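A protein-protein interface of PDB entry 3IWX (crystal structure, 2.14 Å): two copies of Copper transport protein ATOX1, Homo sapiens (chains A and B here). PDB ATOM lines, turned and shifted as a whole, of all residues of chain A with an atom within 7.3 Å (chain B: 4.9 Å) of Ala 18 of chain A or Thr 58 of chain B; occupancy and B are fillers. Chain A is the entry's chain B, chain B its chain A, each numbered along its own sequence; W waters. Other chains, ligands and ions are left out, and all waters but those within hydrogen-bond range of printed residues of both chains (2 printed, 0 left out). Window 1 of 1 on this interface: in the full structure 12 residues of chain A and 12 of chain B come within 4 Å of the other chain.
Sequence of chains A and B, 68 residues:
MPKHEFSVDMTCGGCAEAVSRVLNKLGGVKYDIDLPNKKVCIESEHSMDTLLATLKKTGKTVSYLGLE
N of Lys 60 of chain B lies within hydrogen-bond range of OG1 of Thr 58 of chain B, at 3.1 Å.
The side-chain hydroxyl (OG1) of Thr 58 of chain A is in hydrogen-bond range of the backbone carbonyl oxygen (O) of Leu 55 of chain A (2.6 Å).
The backbone carbonyl oxygen (O) of Leu 55 of chain B sits at hydrogen-bond distance from the side-chain hydroxyl (OG1) of Thr 58 of chain B, at 2.7 Å.
The backbone NH of Gly 14 of chain A lies close to the side-chain sulfur of Cys 12 of chain A (3.3 Å).
The guanidinium group (NH2) of Arg 21 of chain A lies within salt-bridge range of the side-chain carboxylate (OE1) of Glu 17 of chain A.
The side-chain amino group (NZ) of Lys 57 of chain B is in hydrogen-bond range of the backbone carbonyl oxygen (O) of Thr 54 of chain B, 3.0 Å away.
The backbone carbonyl oxygen (O) of Lys 57 of chain A lies close to the backbone carbonyl oxygen (O) of Lys 57 of chain B, 3.2 Å away.
The guanidinium group (NH1) of Arg 21 of chain A is in hydrogen-bond range of the backbone carbonyl oxygen (O) of Gly 59 of chain B, 3.0 Å away.
NZ of Lys 60 of chain B is in hydrogen-bond range of O of Gly 14 of chain A (3.3 Å).
Of the 10 printed residues of chain B, 6 touch a printed residue of chain A.
Hydrophobic or aromatic side chains of chain B that line the printed part of chain A: Ala 18 and Val 22.
Along chain B the printed residues that touch a printed residue of chain A span positions 18 to 60.
Among the printed residues, 14 pairs touch across the chains.
Among the printed residues, no Asp or Glu carboxylate lies within 4 Å of a Lys or Arg side-chain nitrogen of the other chain.
Ala 18 of chain A touches Thr 58 of chain B (CB to O, 3.3 Å).
Ala 18 of chain A touches Gly 59 of chain B.
Val 22 of chain A touches Lys 57 of chain B.
Lys 57 of chain A touches Val 22 of chain B.
O of Lys 57 of chain A touches N of Thr 58 of chain B, 3.9 Å away.
Ala 18 of chain B touches Thr 58 of chain A (CB to O, 3.4 Å).
Thr 58 of chain A touches Lys 57 of chain B (N to O, 3.7 Å).
Thr 58 of chain B touches Thr 58 of chain A.
Gly 59 of chain A touches Ala 18 of chain B (O to CA, 3.6 Å).
CG1 of Val 22 of chain B touches CA of Gly 59 of chain A, at 3.7 Å.
Ala 18 of chain A touches Thr 58 of chain B, and with the chains exchanged Thr 58 of chain A touches Ala 18 of chain B.
Val 22 of chain A touches Lys 57 of chain B, and with the chains exchanged Lys 57 of chain A touches Val 22 of chain B.
Lys 57 of chain A touches its own counterpart, Lys 57 of chain B.
Lys 57 of chain A touches Thr 58 of chain B, and with the chains exchanged Thr 58 of chain A touches Lys 57 of chain B.
Of the 14 pairs that touch across the chains among the printed residues, 12 have their exchanged pair printed and touching as well.
Gly 13 of chain A touches none of the printed residues of chain B.
Of the printed residues of chain B, Ala 18 of chain A touches Thr 58 and Gly 59.
Of the printed residues of chain B, Val 22 of chain A touches Lys 57 (3.5 Å) and Gly 59 (3.8 Å).
Of the printed residues of chain B, Gly 59 of chain A touches Ala 18 (3.6 Å) and Val 22 (3.7 Å).
Printed residues of chain A within 4 Å of Val 22 of chain B: Lys 57 and Gly 59.
Lys 56 of chain B touches none of the printed residues of chain A.
Of the printed residues of chain A, Lys 57 of chain B touches Val 22, Lys 57 and Thr 58.
Thr 58 of chain B touches just these residues of chain A: Ala 18 (3.3 Å), Lys 57 (3.9 Å) and Thr 58 (3.6 Å).
Printed residues of chain A within 4 Å of Lys 60 of chain B: Gly 14.
The nearest residue of chain B that does not touch Ala 18 of chain A is Lys 60 of chain B (4.2 Å).
The nearest residue of chain A that does not touch Thr 58 of chain B is Val 22 of chain A (4.2 Å).
Water W1 lies within hydrogen-bond range of the backbone carbonyl oxygen (O) of Thr 58 of chain B, the backbone carbonyl oxygen (O) of Thr 58 of chain A and the side-chain amino group (NZ) of Lys 60 of chain A.
Water W2 lies within hydrogen-bond range of the guanidinium group (NH1) of Arg 21 of chain A (2.7 Å), the side-chain amino group (NZ) of Lys 60 of chain B (2.9 Å), the side-chain carboxylate (OE1) of Glu 17 of chain A (3.0 Å) and the backbone carbonyl oxygen (O) of Gly 14 of chain A (3.4 Å).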
ATOM      1  N   CYS A  12      -7.992  13.661   7.695  1.00  0.00           N
ATOM      2  CA  CYS A  12      -9.038  14.444   8.357  1.00  0.00           C
ATOM      3  C   CYS A  12      -8.795  14.510   9.858  1.00  0.00           C
ATOM      4  O   CYS A  12      -7.899  13.857  10.371  1.00  0.00           O
ATOM      5  CB  CYS A  12     -10.443  13.909   8.032  1.00  0.00           C
ATOM      6  SG  CYS A  12     -10.955  12.444   8.981  1.00  0.00           S
ATOM      7  N   GLY A  13      -9.598  15.310  10.547  1.00  0.00           N
ATOM      8  CA  GLY A  13      -9.523  15.418  11.999  1.00  0.00           C
ATOM      9  C   GLY A  13      -9.767  14.090  12.694  1.00  0.00           C
ATOM     10  O   GLY A  13      -9.132  13.799  13.699  1.00  0.00           O
ATOM     11  N   GLY A  14     -10.695  13.291  12.162  1.00  0.00           N
ATOM     12  CA  GLY A  14     -10.913  11.911  12.645  1.00  0.00           C
ATOM     13  C   GLY A  14      -9.647  11.049  12.666  1.00  0.00           C
ATOM     14  O   GLY A  14      -9.469  10.230  13.577  1.00  0.00           O
ATOM     15  N   CYS A  15      -8.777  11.232  11.663  1.00  0.00           N
ATOM     16  CA  CYS A  15      -7.493  10.523  11.577  1.00  0.00           C
ATOM     17  C   CYS A  15      -6.529  10.984  12.683  1.00  0.00           C
ATOM     18  O   CYS A  15      -5.821  10.172  13.293  1.00  0.00           O
ATOM     19  CB  CYS A  15      -6.839  10.728  10.200  1.00  0.00           C
ATOM     20  SG  CYS A  15      -7.773  10.105   8.764  1.00  0.00           S
ATOM     21  N   ALA A  16      -6.502  12.291  12.932  1.00  0.00           N
ATOM     22  CA  ALA A  16      -5.717  12.851  14.041  1.00  0.00           C
ATOM     23  C   ALA A  16      -6.187  12.350  15.417  1.00  0.00           C
ATOM     24  O   ALA A  16      -5.366  12.116  16.316  1.00  0.00           O
ATOM     25  CB  ALA A  16      -5.723  14.379  13.982  1.00  0.00           C
ATOM     26  N   GLU A  17      -7.502  12.185  15.575  1.00  0.00           N
ATOM     27  CA  GLU A  17      -8.058  11.688  16.834  1.00  0.00           C
ATOM     28  C   GLU A  17      -7.635  10.244  17.079  1.00  0.00           C
ATOM     29  O   GLU A  17      -7.290   9.880  18.197  1.00  0.00           O
ATOM     30  CB  GLU A  17      -9.586  11.790  16.853  1.00  0.00           C
ATOM     31  CG  GLU A  17     -10.127  13.214  16.933  1.00  0.00           C
ATOM     32  CD  GLU A  17     -11.641  13.269  16.804  1.00  0.00           C
ATOM     33  OE1 GLU A  17     -12.275  12.214  16.618  1.00  0.00           O
ATOM     34  OE2 GLU A  17     -12.202  14.369  16.884  1.00  0.00           O
ATOM     35  N   ALA A  18      -7.655   9.437  16.018  1.00  0.00           N
ATOM     36  CA  ALA A  18      -7.274   8.031  16.086  1.00  0.00           C
ATOM     37  C   ALA A  18      -5.818   7.861  16.542  1.00  0.00           C
ATOM     38  O   ALA A  18      -5.514   7.013  17.388  1.00  0.00           O
ATOM     39  CB  ALA A  18      -7.497   7.362  14.729  1.00  0.00           C
ATOM     40  N   VAL A  19      -4.932   8.666  15.964  1.00  0.00           N
ATOM     41  CA  VAL A  19      -3.535   8.731  16.381  1.00  0.00           C
ATOM     42  C   VAL A  19      -3.454   9.118  17.865  1.00  0.00           C
ATOM     43  O   VAL A  19      -2.771   8.461  18.648  1.00  0.00           O
ATOM     44  CB  VAL A  19      -2.743   9.739  15.517  1.00  0.00           C
ATOM     45  CG1 VAL A  19      -1.343   9.987  16.105  1.00  0.00           C
ATOM     46  CG2 VAL A  19      -2.641   9.230  14.071  1.00  0.00           C
ATOM     47  N   SER A  20      -4.178  10.168  18.245  1.00  0.00           N
ATOM     48  CA  SER A  20      -4.258  10.565  19.640  1.00  0.00           C
ATOM     49  C   SER A  20      -4.707   9.412  20.556  1.00  0.00           C
ATOM     50  O   SER A  20      -4.114   9.204  21.616  1.00  0.00           O
ATOM     51  CB  SER A  20      -5.183  11.770  19.813  1.00  0.00           C
ATOM     52  OG  SER A  20      -5.442  11.971  21.182  1.00  0.00           O
ATOM     53  N   ARG A  21      -5.739   8.669  20.146  1.00  0.00           N
ATOM     54  CA  ARG A  21      -6.260   7.567  20.961  1.00  0.00           C
ATOM     55  C   ARG A  21      -5.252   6.433  21.153  1.00  0.00           C
ATOM     56  O   ARG A  21      -5.136   5.894  22.256  1.00  0.00           O
ATOM     57  CB  ARG A  21      -7.583   7.012  20.401  1.00  0.00           C
ATOM     58  CG  ARG A  21      -8.783   7.934  20.588  1.00  0.00           C
ATOM     59  CD  ARG A  21     -10.103   7.155  20.424  1.00  0.00           C
ATOM     60  NE  ARG A  21     -11.268   8.034  20.316  1.00  0.00           N
ATOM     61  CZ  ARG A  21     -11.675   8.651  19.202  1.00  0.00           C
ATOM     62  NH1 ARG A  21     -11.024   8.506  18.047  1.00  0.00           N
ATOM     63  NH2 ARG A  21     -12.751   9.422  19.243  1.00  0.00           N
ATOM     64  N   VAL A  22      -4.533   6.058  20.093  1.00  0.00           N
ATOM     65  CA  VAL A  22      -3.540   4.969  20.216  1.00  0.00           C
ATOM     66  C   VAL A  22      -2.319   5.371  21.062  1.00  0.00           C
ATOM     67  O   VAL A  22      -1.800   4.559  21.836  1.00  0.00           O
ATOM     68  CB  VAL A  22      -3.133   4.330  18.854  1.00  0.00           C
ATOM     69  CG1 VAL A  22      -4.374   3.815  18.112  1.00  0.00           C
ATOM     70  CG2 VAL A  22      -2.340   5.305  17.984  1.00  0.00           C
ATOM     71  N   LEU A  23      -1.891   6.626  20.939  1.00  0.00           N
ATOM     72  CA  LEU A  23      -0.790   7.133  21.747  1.00  0.00           C
ATOM     73  C   LEU A  23      -1.181   7.264  23.222  1.00  0.00           C
ATOM     74  O   LEU A  23      -0.403   6.881  24.097  1.00  0.00           O
ATOM     75  CB  LEU A  23      -0.253   8.453  21.193  1.00  0.00           C
ATOM     76  CG  LEU A  23       0.416   8.395  19.819  1.00  0.00           C
ATOM     77  CD1 LEU A  23       0.889   9.789  19.370  1.00  0.00           C
ATOM     78  CD2 LEU A  23       1.573   7.370  19.792  1.00  0.00           C
ATOM     79  N   ASN A  24      -2.379   7.782  23.498  1.00  0.00           N
ATOM     80  CA  ASN A  24      -2.916   7.794  24.862  1.00  0.00           C
ATOM     81  C   ASN A  24      -2.956   6.394  25.477  1.00  0.00           C
ATOM     82  O   ASN A  24      -2.607   6.217  26.645  1.00  0.00           O
ATOM     83  CB  ASN A  24      -4.329   8.390  24.910  1.00  0.00           C
ATOM     84  CG  ASN A  24      -4.357   9.897  24.661  1.00  0.00           C
ATOM     85  OD1 ASN A  24      -5.432  10.471  24.473  1.00  0.00           O
ATOM     86  ND2 ASN A  24      -3.187  10.541  24.657  1.00  0.00           N
ATOM     87  N   ILE A  33       0.417  16.678  17.174  1.00  0.00           N
ATOM     88  CA  ILE A  33      -0.014  16.190  15.883  1.00  0.00           C
ATOM     89  C   ILE A  33      -0.259  17.386  14.970  1.00  0.00           C
ATOM     90  O   ILE A  33      -1.113  18.232  15.260  1.00  0.00           O
ATOM     91  CB  ILE A  33      -1.315  15.348  16.014  1.00  0.00           C
ATOM     92  CG1 ILE A  33      -1.083  14.100  16.886  1.00  0.00           C
ATOM     93  CG2 ILE A  33      -1.874  14.982  14.634  1.00  0.00           C
ATOM     94  CD1 ILE A  33      -2.393  13.460  17.413  1.00  0.00           C
ATOM     95  N   THR A  54       3.152   1.246  17.444  1.00  0.00           N
ATOM     96  CA  THR A  54       1.925   1.857  17.972  1.00  0.00           C
ATOM     97  C   THR A  54       1.209   2.710  16.909  1.00  0.00           C
ATOM     98  O   THR A  54      -0.009   2.614  16.743  1.00  0.00           O
ATOM     99  CB  THR A  54       2.229   2.726  19.214  1.00  0.00           C
ATOM    100  OG1 THR A  54       2.870   1.925  20.211  1.00  0.00           O
ATOM    101  CG2 THR A  54       0.951   3.335  19.812  1.00  0.00           C
ATOM    102  N   LEU A  55       1.974   3.529  16.191  1.00  0.00           N
ATOM    103  CA  LEU A  55       1.435   4.328  15.088  1.00  0.00           C
ATOM    104  C   LEU A  55       0.935   3.460  13.941  1.00  0.00           C
ATOM    105  O   LEU A  55      -0.114   3.737  13.377  1.00  0.00           O
ATOM    106  CB  LEU A  55       2.474   5.350  14.580  1.00  0.00           C
ATOM    107  CG  LEU A  55       2.854   6.459  15.562  1.00  0.00           C
ATOM    108  CD1 LEU A  55       4.001   7.269  14.991  1.00  0.00           C
ATOM    109  CD2 LEU A  55       1.667   7.390  15.921  1.00  0.00           C
ATOM    110  N   LYS A  57      -0.374   0.729  14.079  1.00  0.00           N
ATOM    111  CA  LYS A  57      -1.594   0.054  14.525  1.00  0.00           C
ATOM    112  C   LYS A  57      -2.850   0.676  13.933  1.00  0.00           C
ATOM    113  O   LYS A  57      -3.834  -0.021  13.688  1.00  0.00           O
ATOM    114  CB  LYS A  57      -1.704   0.091  16.055  1.00  0.00           C
ATOM    115  CG  LYS A  57      -1.031  -1.078  16.723  1.00  0.00           C
ATOM    116  CD  LYS A  57      -1.129  -1.011  18.245  1.00  0.00           C
ATOM    117  CE  LYS A  57      -0.404  -2.224  18.834  1.00  0.00           C
ATOM    118  NZ  LYS A  57      -0.564  -2.367  20.306  1.00  0.00           N
ATOM    119  N   THR A  58      -2.813   1.990  13.737  1.00  0.00           N
ATOM    120  CA  THR A  58      -3.930   2.745  13.179  1.00  0.00           C
ATOM    121  C   THR A  58      -4.319   2.212  11.800  1.00  0.00           C
ATOM    122  O   THR A  58      -5.445   2.432  11.344  1.00  0.00           O
ATOM    123  CB  THR A  58      -3.553   4.223  12.998  1.00  0.00           C
ATOM    124  OG1 THR A  58      -2.373   4.306  12.197  1.00  0.00           O
ATOM    125  CG2 THR A  58      -3.298   4.913  14.343  1.00  0.00           C
ATOM    126  N   GLY A  59      -3.378   1.527  11.145  1.00  0.00           N
ATOM    127  CA  GLY A  59      -3.530   1.093   9.757  1.00  0.00           C
ATOM    128  C   GLY A  59      -3.246   2.198   8.740  1.00  0.00           C
ATOM    129  O   GLY A  59      -3.514   2.034   7.549  1.00  0.00           O
ATOM    130  N   LYS A  60      -2.716   3.323   9.225  1.00  0.00           N
ATOM    131  CA  LYS A  60      -2.273   4.427   8.377  1.00  0.00           C
ATOM    132  C   LYS A  60      -0.811   4.226   7.968  1.00  0.00           C
ATOM    133  O   LYS A  60      -0.062   3.501   8.639  1.00  0.00           O
ATOM    134  CB  LYS A  60      -2.444   5.756   9.121  1.00  0.00           C
ATOM    135  CG  LYS A  60      -3.896   6.029   9.534  1.00  0.00           C
ATOM    136  CD  LYS A  60      -4.016   7.271  10.394  1.00  0.00           C
ATOM    137  CE  LYS A  60      -5.273   7.228  11.264  1.00  0.00           C
ATOM    138  NZ  LYS A  60      -6.489   6.814  10.496  1.00  0.00           N
ATOM    139  N   ALA B  18      -7.780   2.716   6.275  1.00  0.00           N
ATOM    140  CA  ALA B  18      -7.074   2.252   7.479  1.00  0.00           C
ATOM    141  C   ALA B  18      -7.766   1.041   8.087  1.00  0.00           C
ATOM    142  O   ALA B  18      -7.101   0.110   8.552  1.00  0.00           O
ATOM    143  CB  ALA B  18      -6.963   3.366   8.499  1.00  0.00           C
ATOM    144  N   VAL B  19      -9.100   1.049   8.075  1.00  0.00           N
ATOM    145  CA  VAL B  19      -9.876  -0.106   8.526  1.00  0.00           C
ATOM    146  C   VAL B  19      -9.562  -1.340   7.682  1.00  0.00           C
ATOM    147  O   VAL B  19      -9.330  -2.422   8.219  1.00  0.00           O
ATOM    148  CB  VAL B  19     -11.400   0.177   8.512  1.00  0.00           C
ATOM    149  CG1 VAL B  19     -12.184  -1.106   8.694  1.00  0.00           C
ATOM    150  CG2 VAL B  19     -11.752   1.182   9.607  1.00  0.00           C
ATOM    151  N   VAL B  22      -5.996  -2.897   8.602  1.00  0.00           N
ATOM    152  CA  VAL B  22      -5.907  -3.708   9.825  1.00  0.00           C
ATOM    153  C   VAL B  22      -6.636  -5.036   9.639  1.00  0.00           C
ATOM    154  O   VAL B  22      -6.209  -6.065  10.168  1.00  0.00           O
ATOM    155  CB  VAL B  22      -6.363  -2.961  11.120  1.00  0.00           C
ATOM    156  CG1 VAL B  22      -5.605  -1.627  11.270  1.00  0.00           C
ATOM    157  CG2 VAL B  22      -7.880  -2.757  11.158  1.00  0.00           C
ATOM    158  N   THR B  54      -9.410  -6.026  16.752  1.00  0.00           N
ATOM    159  CA  THR B  54      -8.737  -5.666  15.506  1.00  0.00           C
ATOM    160  C   THR B  54      -9.184  -4.285  15.029  1.00  0.00           C
ATOM    161  O   THR B  54      -8.352  -3.431  14.720  1.00  0.00           O
ATOM    162  CB  THR B  54      -8.980  -6.732  14.399  1.00  0.00           C
ATOM    163  OG1 THR B  54      -8.406  -7.979  14.811  1.00  0.00           O
ATOM    164  CG2 THR B  54      -8.360  -6.314  13.069  1.00  0.00           C
ATOM    165  N   LEU B  55     -10.494  -4.061  14.997  1.00  0.00           N
ATOM    166  CA  LEU B  55     -11.036  -2.786  14.555  1.00  0.00           C
ATOM    167  C   LEU B  55     -10.659  -1.662  15.514  1.00  0.00           C
ATOM    168  O   LEU B  55     -10.351  -0.558  15.076  1.00  0.00           O
ATOM    169  CB  LEU B  55     -12.557  -2.862  14.360  1.00  0.00           C
ATOM    170  CG  LEU B  55     -13.076  -3.687  13.173  1.00  0.00           C
ATOM    171  CD1 LEU B  55     -14.590  -3.873  13.257  1.00  0.00           C
ATOM    172  CD2 LEU B  55     -12.687  -3.060  11.819  1.00  0.00           C
ATOM    173  N   LYS B  56     -10.637  -1.960  16.813  1.00  0.00           N
ATOM    174  CA  LYS B  56     -10.339  -0.951  17.820  1.00  0.00           C
ATOM    175  C   LYS B  56      -8.879  -0.460  17.794  1.00  0.00           C
ATOM    176  O   LYS B  56      -8.583   0.615  18.306  1.00  0.00           O
ATOM    177  CB  LYS B  56     -10.719  -1.448  19.212  1.00  0.00           C
ATOM    178  CG  LYS B  56     -12.195  -1.339  19.518  1.00  0.00           C
ATOM    179  CD  LYS B  56     -12.499  -1.971  20.860  1.00  0.00           C
ATOM    180  CE  LYS B  56     -13.896  -1.611  21.345  1.00  0.00           C
ATOM    181  NZ  LYS B  56     -14.135  -2.126  22.730  1.00  0.00           N
ATOM    182  N   LYS B  57      -7.988  -1.244  17.183  1.00  0.00           N
ATOM    183  CA  LYS B  57      -6.587  -0.848  16.984  1.00  0.00           C
ATOM    184  C   LYS B  57      -6.418   0.381  16.091  1.00  0.00           C
ATOM    185  O   LYS B  57      -5.427   1.099  16.210  1.00  0.00           O
ATOM    186  CB  LYS B  57      -5.778  -1.990  16.379  1.00  0.00           C
ATOM    187  CG  LYS B  57      -5.433  -3.097  17.354  1.00  0.00           C
ATOM    188  CD  LYS B  57      -4.294  -3.976  16.843  1.00  0.00           C
ATOM    189  CE  LYS B  57      -4.322  -4.174  15.330  1.00  0.00           C
ATOM    190  NZ  LYS B  57      -5.623  -4.691  14.805  1.00  0.00           N
ATOM    191  N   THR B  58      -7.371   0.619  15.197  1.00  0.00           N
ATOM    192  CA  THR B  58      -7.340   1.814  14.361  1.00  0.00           C
ATOM    193  C   THR B  58      -7.342   3.101  15.192  1.00  0.00           C
ATOM    194  O   THR B  58      -6.922   4.148  14.712  1.00  0.00           O
ATOM    195  CB  THR B  58      -8.529   1.864  13.399  1.00  0.00           C
ATOM    196  OG1 THR B  58      -9.747   1.910  14.153  1.00  0.00           O
ATOM    197  CG2 THR B  58      -8.538   0.637  12.488  1.00  0.00           C
ATOM    198  N   GLY B  59      -7.820   3.012  16.431  1.00  0.00           N
ATOM    199  CA  GLY B  59      -8.033   4.186  17.269  1.00  0.00           C
ATOM    200  C   GLY B  59      -9.377   4.854  17.030  1.00  0.00           C
ATOM    201  O   GLY B  59      -9.657   5.911  17.596  1.00  0.00           O
ATOM    202  N   LYS B  60     -10.212   4.240  16.191  1.00  0.00           N
ATOM    203  CA  LYS B  60     -11.549   4.761  15.917  1.00  0.00           C
ATOM    204  C   LYS B  60     -12.540   4.187  16.922  1.00  0.00           C
ATOM    205  O   LYS B  60     -12.310   3.108  17.469  1.00  0.00           O
ATOM    206  CB  LYS B  60     -12.008   4.378  14.505  1.00  0.00           C
ATOM    207  CG  LYS B  60     -11.183   4.966  13.385  1.00  0.00           C
ATOM    208  CD  LYS B  60     -11.880   6.187  12.738  1.00  0.00           C
ATOM    209  CE  LYS B  60     -11.511   7.501  13.417  1.00  0.00           C
ATOM    210  NZ  LYS B  60     -12.278   8.663  12.844  1.00  0.00           N
HETATM  211  O   HOH W   1      -6.852   4.553  12.137  1.00  0.00           O
HETATM  212  O   HOH W   2     -12.015   9.356  15.645  1.00  0.00           O
